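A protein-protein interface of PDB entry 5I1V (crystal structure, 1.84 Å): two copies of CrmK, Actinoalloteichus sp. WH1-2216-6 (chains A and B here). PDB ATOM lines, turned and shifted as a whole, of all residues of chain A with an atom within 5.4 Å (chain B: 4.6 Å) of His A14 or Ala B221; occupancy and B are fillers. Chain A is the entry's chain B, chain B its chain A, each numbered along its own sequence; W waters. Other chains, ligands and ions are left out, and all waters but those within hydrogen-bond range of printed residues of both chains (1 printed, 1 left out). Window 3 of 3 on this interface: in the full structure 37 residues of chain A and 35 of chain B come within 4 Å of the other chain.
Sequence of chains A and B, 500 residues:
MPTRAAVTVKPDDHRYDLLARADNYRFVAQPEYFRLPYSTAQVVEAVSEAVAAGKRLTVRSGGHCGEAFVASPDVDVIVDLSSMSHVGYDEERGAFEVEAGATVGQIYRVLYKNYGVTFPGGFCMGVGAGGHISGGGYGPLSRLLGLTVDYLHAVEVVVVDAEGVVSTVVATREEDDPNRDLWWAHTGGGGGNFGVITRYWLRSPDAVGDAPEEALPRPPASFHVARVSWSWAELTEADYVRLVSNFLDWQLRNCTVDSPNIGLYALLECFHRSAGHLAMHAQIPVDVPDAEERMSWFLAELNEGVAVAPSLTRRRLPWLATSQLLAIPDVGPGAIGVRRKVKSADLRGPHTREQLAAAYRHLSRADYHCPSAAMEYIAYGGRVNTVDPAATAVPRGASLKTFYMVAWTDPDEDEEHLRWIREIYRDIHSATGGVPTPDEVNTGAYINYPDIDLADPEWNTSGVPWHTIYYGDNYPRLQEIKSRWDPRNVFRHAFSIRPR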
ATOM      1  N   ASP A  12     -18.513 -13.724 -12.212  1.00  0.00           N
ATOM      2  CA  ASP A  12     -17.288 -13.151 -11.642  1.00  0.00           C
ATOM      3  C   ASP A  12     -17.468 -12.655 -10.190  1.00  0.00           C
ATOM      4  O   ASP A  12     -16.517 -12.285  -9.547  1.00  0.00           O
ATOM      5  CB  ASP A  12     -16.765 -12.021 -12.549  1.00  0.00           C
ATOM      6  CG  ASP A  12     -17.692 -10.761 -12.571  1.00  0.00           C
ATOM      7  OD1 ASP A  12     -18.852 -10.779 -12.093  1.00  0.00           O
ATOM      8  OD2 ASP A  12     -17.248  -9.719 -13.091  1.00  0.00           O
ATOM      9  N   ASP A  13     -18.686 -12.649  -9.677  1.00  0.00           N
ATOM     10  CA  ASP A  13     -18.997 -12.207  -8.311  1.00  0.00           C
ATOM     11  C   ASP A  13     -18.876 -13.440  -7.431  1.00  0.00           C
ATOM     12  O   ASP A  13     -19.370 -14.490  -7.784  1.00  0.00           O
ATOM     13  CB  ASP A  13     -20.424 -11.708  -8.281  1.00  0.00           C
ATOM     14  CG  ASP A  13     -20.806 -11.027  -6.987  1.00  0.00           C
ATOM     15  OD1 ASP A  13     -20.815 -11.651  -5.884  1.00  0.00           O
ATOM     16  OD2 ASP A  13     -21.141  -9.818  -7.078  1.00  0.00           O
ATOM     17  N   HIS A  14     -18.247 -13.299  -6.278  1.00  0.00           N
ATOM     18  CA  HIS A  14     -18.108 -14.406  -5.313  1.00  0.00           C
ATOM     19  C   HIS A  14     -19.425 -15.010  -4.860  1.00  0.00           C
ATOM     20  O   HIS A  14     -19.502 -16.188  -4.473  1.00  0.00           O
ATOM     21  CB  HIS A  14     -17.328 -13.923  -4.084  1.00  0.00           C
ATOM     22  CG  HIS A  14     -15.894 -13.650  -4.376  1.00  0.00           C
ATOM     23  ND1 HIS A  14     -15.072 -12.963  -3.511  1.00  0.00           N
ATOM     24  CD2 HIS A  14     -15.136 -13.963  -5.452  1.00  0.00           C
ATOM     25  CE1 HIS A  14     -13.865 -12.871  -4.041  1.00  0.00           C
ATOM     26  NE2 HIS A  14     -13.880 -13.465  -5.221  1.00  0.00           N
ATOM     27  N   ARG A  15     -20.474 -14.213  -4.885  1.00  0.00           N
ATOM     28  CA  ARG A  15     -21.812 -14.733  -4.531  1.00  0.00           C
ATOM     29  C   ARG A  15     -22.381 -15.760  -5.460  1.00  0.00           C
ATOM     30  O   ARG A  15     -23.271 -16.486  -5.063  1.00  0.00           O
ATOM     31  CB  ARG A  15     -22.840 -13.610  -4.417  1.00  0.00           C
ATOM     32  CG  ARG A  15     -22.576 -12.829  -3.152  1.00  0.00           C
ATOM     33  CD  ARG A  15     -23.443 -11.602  -3.113  1.00  0.00           C
ATOM     34  NE  ARG A  15     -22.995 -10.676  -4.123  1.00  0.00           N
ATOM     35  CZ  ARG A  15     -23.489  -9.445  -4.255  1.00  0.00           C
ATOM     36  NH1 ARG A  15     -24.493  -9.043  -3.502  1.00  0.00           N
ATOM     37  NH2 ARG A  15     -23.018  -8.646  -5.179  1.00  0.00           N
ATOM     38  N   TYR A  16     -21.893 -15.809  -6.698  1.00  0.00           N
ATOM     39  CA  TYR A  16     -22.530 -16.628  -7.725  1.00  0.00           C
ATOM     40  C   TYR A  16     -22.550 -18.098  -7.347  1.00  0.00           C
ATOM     41  O   TYR A  16     -23.567 -18.771  -7.492  1.00  0.00           O
ATOM     42  CB  TYR A  16     -21.805 -16.455  -9.043  1.00  0.00           C
ATOM     43  CG  TYR A  16     -22.399 -17.188 -10.226  1.00  0.00           C
ATOM     44  CD1 TYR A  16     -22.102 -18.532 -10.477  1.00  0.00           C
ATOM     45  CD2 TYR A  16     -23.257 -16.531 -11.109  1.00  0.00           C
ATOM     46  CE1 TYR A  16     -22.646 -19.176 -11.611  1.00  0.00           C
ATOM     47  CE2 TYR A  16     -23.799 -17.168 -12.214  1.00  0.00           C
ATOM     48  CZ  TYR A  16     -23.482 -18.501 -12.454  1.00  0.00           C
ATOM     49  OH  TYR A  16     -24.007 -19.149 -13.545  1.00  0.00           O
ATOM     50  N   ASP A  17     -21.444 -18.613  -6.880  1.00  0.00           N
ATOM     51  CA  ASP A  17     -21.364 -20.049  -6.597  1.00  0.00           C
ATOM     52  C   ASP A  17     -22.288 -20.474  -5.453  1.00  0.00           C
ATOM     53  O   ASP A  17     -22.770 -21.620  -5.385  1.00  0.00           O
ATOM     54  CB  ASP A  17     -19.927 -20.444  -6.269  1.00  0.00           C
ATOM     55  CG  ASP A  17     -19.047 -20.550  -7.524  1.00  0.00           C
ATOM     56  OD1 ASP A  17     -19.603 -20.626  -8.653  1.00  0.00           O
ATOM     57  OD2 ASP A  17     -17.800 -20.563  -7.399  1.00  0.00           O
ATOM     58  N   LEU A  18     -22.521 -19.558  -4.532  1.00  0.00           N
ATOM     59  CA  LEU A  18     -23.433 -19.827  -3.428  1.00  0.00           C
ATOM     60  C   LEU A  18     -24.873 -19.850  -3.953  1.00  0.00           C
ATOM     61  O   LEU A  18     -25.660 -20.769  -3.670  1.00  0.00           O
ATOM     62  CB  LEU A  18     -23.237 -18.768  -2.355  1.00  0.00           C
ATOM     63  CG  LEU A  18     -24.022 -18.826  -1.030  1.00  0.00           C
ATOM     64  CD1 LEU A  18     -25.345 -18.075  -1.151  1.00  0.00           C
ATOM     65  CD2 LEU A  18     -24.244 -20.237  -0.506  1.00  0.00           C
ATOM     66  N   TYR B 112     -24.615 -11.213   3.407  1.00  0.00           N
ATOM     67  CA  TYR B 112     -23.891 -11.860   2.393  1.00  0.00           C
ATOM     68  C   TYR B 112     -24.616 -11.827   1.057  1.00  0.00           C
ATOM     69  O   TYR B 112     -24.039 -11.430   0.074  1.00  0.00           O
ATOM     70  CB  TYR B 112     -23.527 -13.319   2.782  1.00  0.00           C
ATOM     71  CG  TYR B 112     -22.564 -13.837   1.753  1.00  0.00           C
ATOM     72  CD1 TYR B 112     -21.256 -13.396   1.721  1.00  0.00           C
ATOM     73  CD2 TYR B 112     -23.008 -14.661   0.715  1.00  0.00           C
ATOM     74  CE1 TYR B 112     -20.373 -13.830   0.734  1.00  0.00           C
ATOM     75  CE2 TYR B 112     -22.140 -15.096  -0.273  1.00  0.00           C
ATOM     76  CZ  TYR B 112     -20.832 -14.705  -0.271  1.00  0.00           C
ATOM     77  OH  TYR B 112     -20.024 -15.171  -1.301  1.00  0.00           O
ATOM     78  N   PRO B 219     -15.920 -12.181   2.982  1.00  0.00           N
ATOM     79  CA  PRO B 219     -15.209 -13.419   3.382  1.00  0.00           C
ATOM     80  C   PRO B 219     -14.519 -14.076   2.178  1.00  0.00           C
ATOM     81  O   PRO B 219     -14.766 -13.668   1.036  1.00  0.00           O
ATOM     82  CB  PRO B 219     -16.333 -14.292   3.889  1.00  0.00           C
ATOM     83  CG  PRO B 219     -17.530 -13.888   3.047  1.00  0.00           C
ATOM     84  CD  PRO B 219     -17.353 -12.411   2.782  1.00  0.00           C
ATOM     85  N   PRO B 220     -13.666 -15.086   2.411  1.00  0.00           N
ATOM     86  CA  PRO B 220     -13.098 -15.867   1.291  1.00  0.00           C
ATOM     87  C   PRO B 220     -14.224 -16.542   0.495  1.00  0.00           C
ATOM     88  O   PRO B 220     -15.234 -16.910   1.065  1.00  0.00           O
ATOM     89  CB  PRO B 220     -12.225 -16.897   2.001  1.00  0.00           C
ATOM     90  CG  PRO B 220     -11.865 -16.219   3.294  1.00  0.00           C
ATOM     91  CD  PRO B 220     -13.143 -15.559   3.703  1.00  0.00           C
ATOM     92  N   ALA B 221     -14.101 -16.636  -0.809  1.00  0.00           N
ATOM     93  CA  ALA B 221     -15.225 -17.117  -1.607  1.00  0.00           C
ATOM     94  C   ALA B 221     -15.539 -18.590  -1.324  1.00  0.00           C
ATOM     95  O   ALA B 221     -16.680 -18.969  -1.329  1.00  0.00           O
ATOM     96  CB  ALA B 221     -14.964 -16.891  -3.091  1.00  0.00           C
ATOM     97  N   SER B 222     -14.524 -19.400  -1.053  1.00  0.00           N
ATOM     98  CA  SER B 222     -14.772 -20.824  -0.845  1.00  0.00           C
ATOM     99  C   SER B 222     -13.642 -21.437  -0.070  1.00  0.00           C
ATOM    100  O   SER B 222     -12.571 -20.815   0.043  1.00  0.00           O
ATOM    101  CB  SER B 222     -15.048 -21.559  -2.154  1.00  0.00           C
ATOM    102  OG  SER B 222     -13.885 -21.865  -2.829  1.00  0.00           O
ATOM    103  N   LEU B 317     -16.473 -26.043  -0.561  1.00  0.00           N
ATOM    104  CA  LEU B 317     -17.804 -25.454  -0.508  1.00  0.00           C
ATOM    105  C   LEU B 317     -17.730 -23.943  -0.532  1.00  0.00           C
ATOM    106  O   LEU B 317     -16.724 -23.364  -0.103  1.00  0.00           O
ATOM    107  CB  LEU B 317     -18.529 -25.900   0.754  1.00  0.00           C
ATOM    108  CG  LEU B 317     -19.159 -27.294   0.785  1.00  0.00           C
ATOM    109  CD1 LEU B 317     -19.765 -27.521   2.143  1.00  0.00           C
ATOM    110  CD2 LEU B 317     -20.223 -27.437  -0.299  1.00  0.00           C
ATOM    111  N   PRO B 318     -18.801 -23.288  -0.997  1.00  0.00           N
ATOM    112  CA  PRO B 318     -18.767 -21.825  -0.849  1.00  0.00           C
ATOM    113  C   PRO B 318     -18.768 -21.413   0.631  1.00  0.00           C
ATOM    114  O   PRO B 318     -19.230 -22.172   1.482  1.00  0.00           O
ATOM    115  CB  PRO B 318     -20.029 -21.371  -1.576  1.00  0.00           C
ATOM    116  CG  PRO B 318     -20.278 -22.427  -2.611  1.00  0.00           C
ATOM    117  CD  PRO B 318     -19.900 -23.718  -1.883  1.00  0.00           C
ATOM    118  N   TRP B 319     -18.241 -20.238   0.943  1.00  0.00           N
ATOM    119  CA  TRP B 319     -18.179 -19.777   2.340  1.00  0.00           C
ATOM    120  C   TRP B 319     -19.492 -19.916   3.141  1.00  0.00           C
ATOM    121  O   TRP B 319     -19.524 -20.543   4.209  1.00  0.00           O
ATOM    122  CB  TRP B 319     -17.667 -18.312   2.468  1.00  0.00           C
ATOM    123  CG  TRP B 319     -17.886 -17.881   3.902  1.00  0.00           C
ATOM    124  CD1 TRP B 319     -17.205 -18.323   4.977  1.00  0.00           C
ATOM    125  CD2 TRP B 319     -18.944 -17.051   4.406  1.00  0.00           C
ATOM    126  NE1 TRP B 319     -17.751 -17.817   6.116  1.00  0.00           N
ATOM    127  CE2 TRP B 319     -18.809 -17.016   5.795  1.00  0.00           C
ATOM    128  CE3 TRP B 319     -19.955 -16.295   3.808  1.00  0.00           C
ATOM    129  CZ2 TRP B 319     -19.671 -16.292   6.614  1.00  0.00           C
ATOM    130  CZ3 TRP B 319     -20.814 -15.563   4.620  1.00  0.00           C
ATOM    131  CH2 TRP B 319     -20.680 -15.581   6.001  1.00  0.00           C
HETATM  132  O   HOH W   1     -16.827 -13.711  -0.843  1.00  0.00           O
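Water W1 bridges the backbone carbonyl oxygen (O) of Pro B219 (2.8 Å) and a ring nitrogen (ND1) of His A14 (3.3 Å).
Of the 8 printed residues of chain B, 3 touch a printed residue of chain A.
Printed residues of chain A that touch a printed residue of chain B: His A14, Arg A15 and Asp A17.
Hydrophobic or aromatic side chains of chain A that line the printed part of chain B: His A14.
Among the printed residues, 4 pairs touch across the chains.
Among the printed residues, no Asp or Glu carboxylate lies within 4 Å of a Lys or Arg side-chain nitrogen of the other chain.
CB of Ala B221 touches CG of His A14, at 3.6 Å.
Arg A15 touches Tyr B112 (CD to O, 3.2 Å).
CG of Pro B318 touches O of Asp A17, at 3.8 Å.
OH of Tyr B112 sits at hydrogen-bond distance from O of His A14 (3.4 Å).
OD2 of Asp A13 lies within salt-bridge range of NH2 of Arg A15, 2.9 Å away.
The backbone carbonyl oxygen (O) of Ala B221 is in hydrogen-bond range of the backbone NH (N) of Trp B319, 3.0 Å away.
His A14 touches just these residues of chain B: Tyr B112 and Ala B221.
Printed residues of chain B within 4 Å of Arg A15: Tyr B112.
Of the printed residues of chain B, Asp A17 touches Pro B318.
Ala B221 touches just one residue of chain A: His A14 (3.6 Å).
The nearest printed residue of chain B that does not touch His A14 is Pro B219 (4.6 Å).
No position is printed for both chains.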
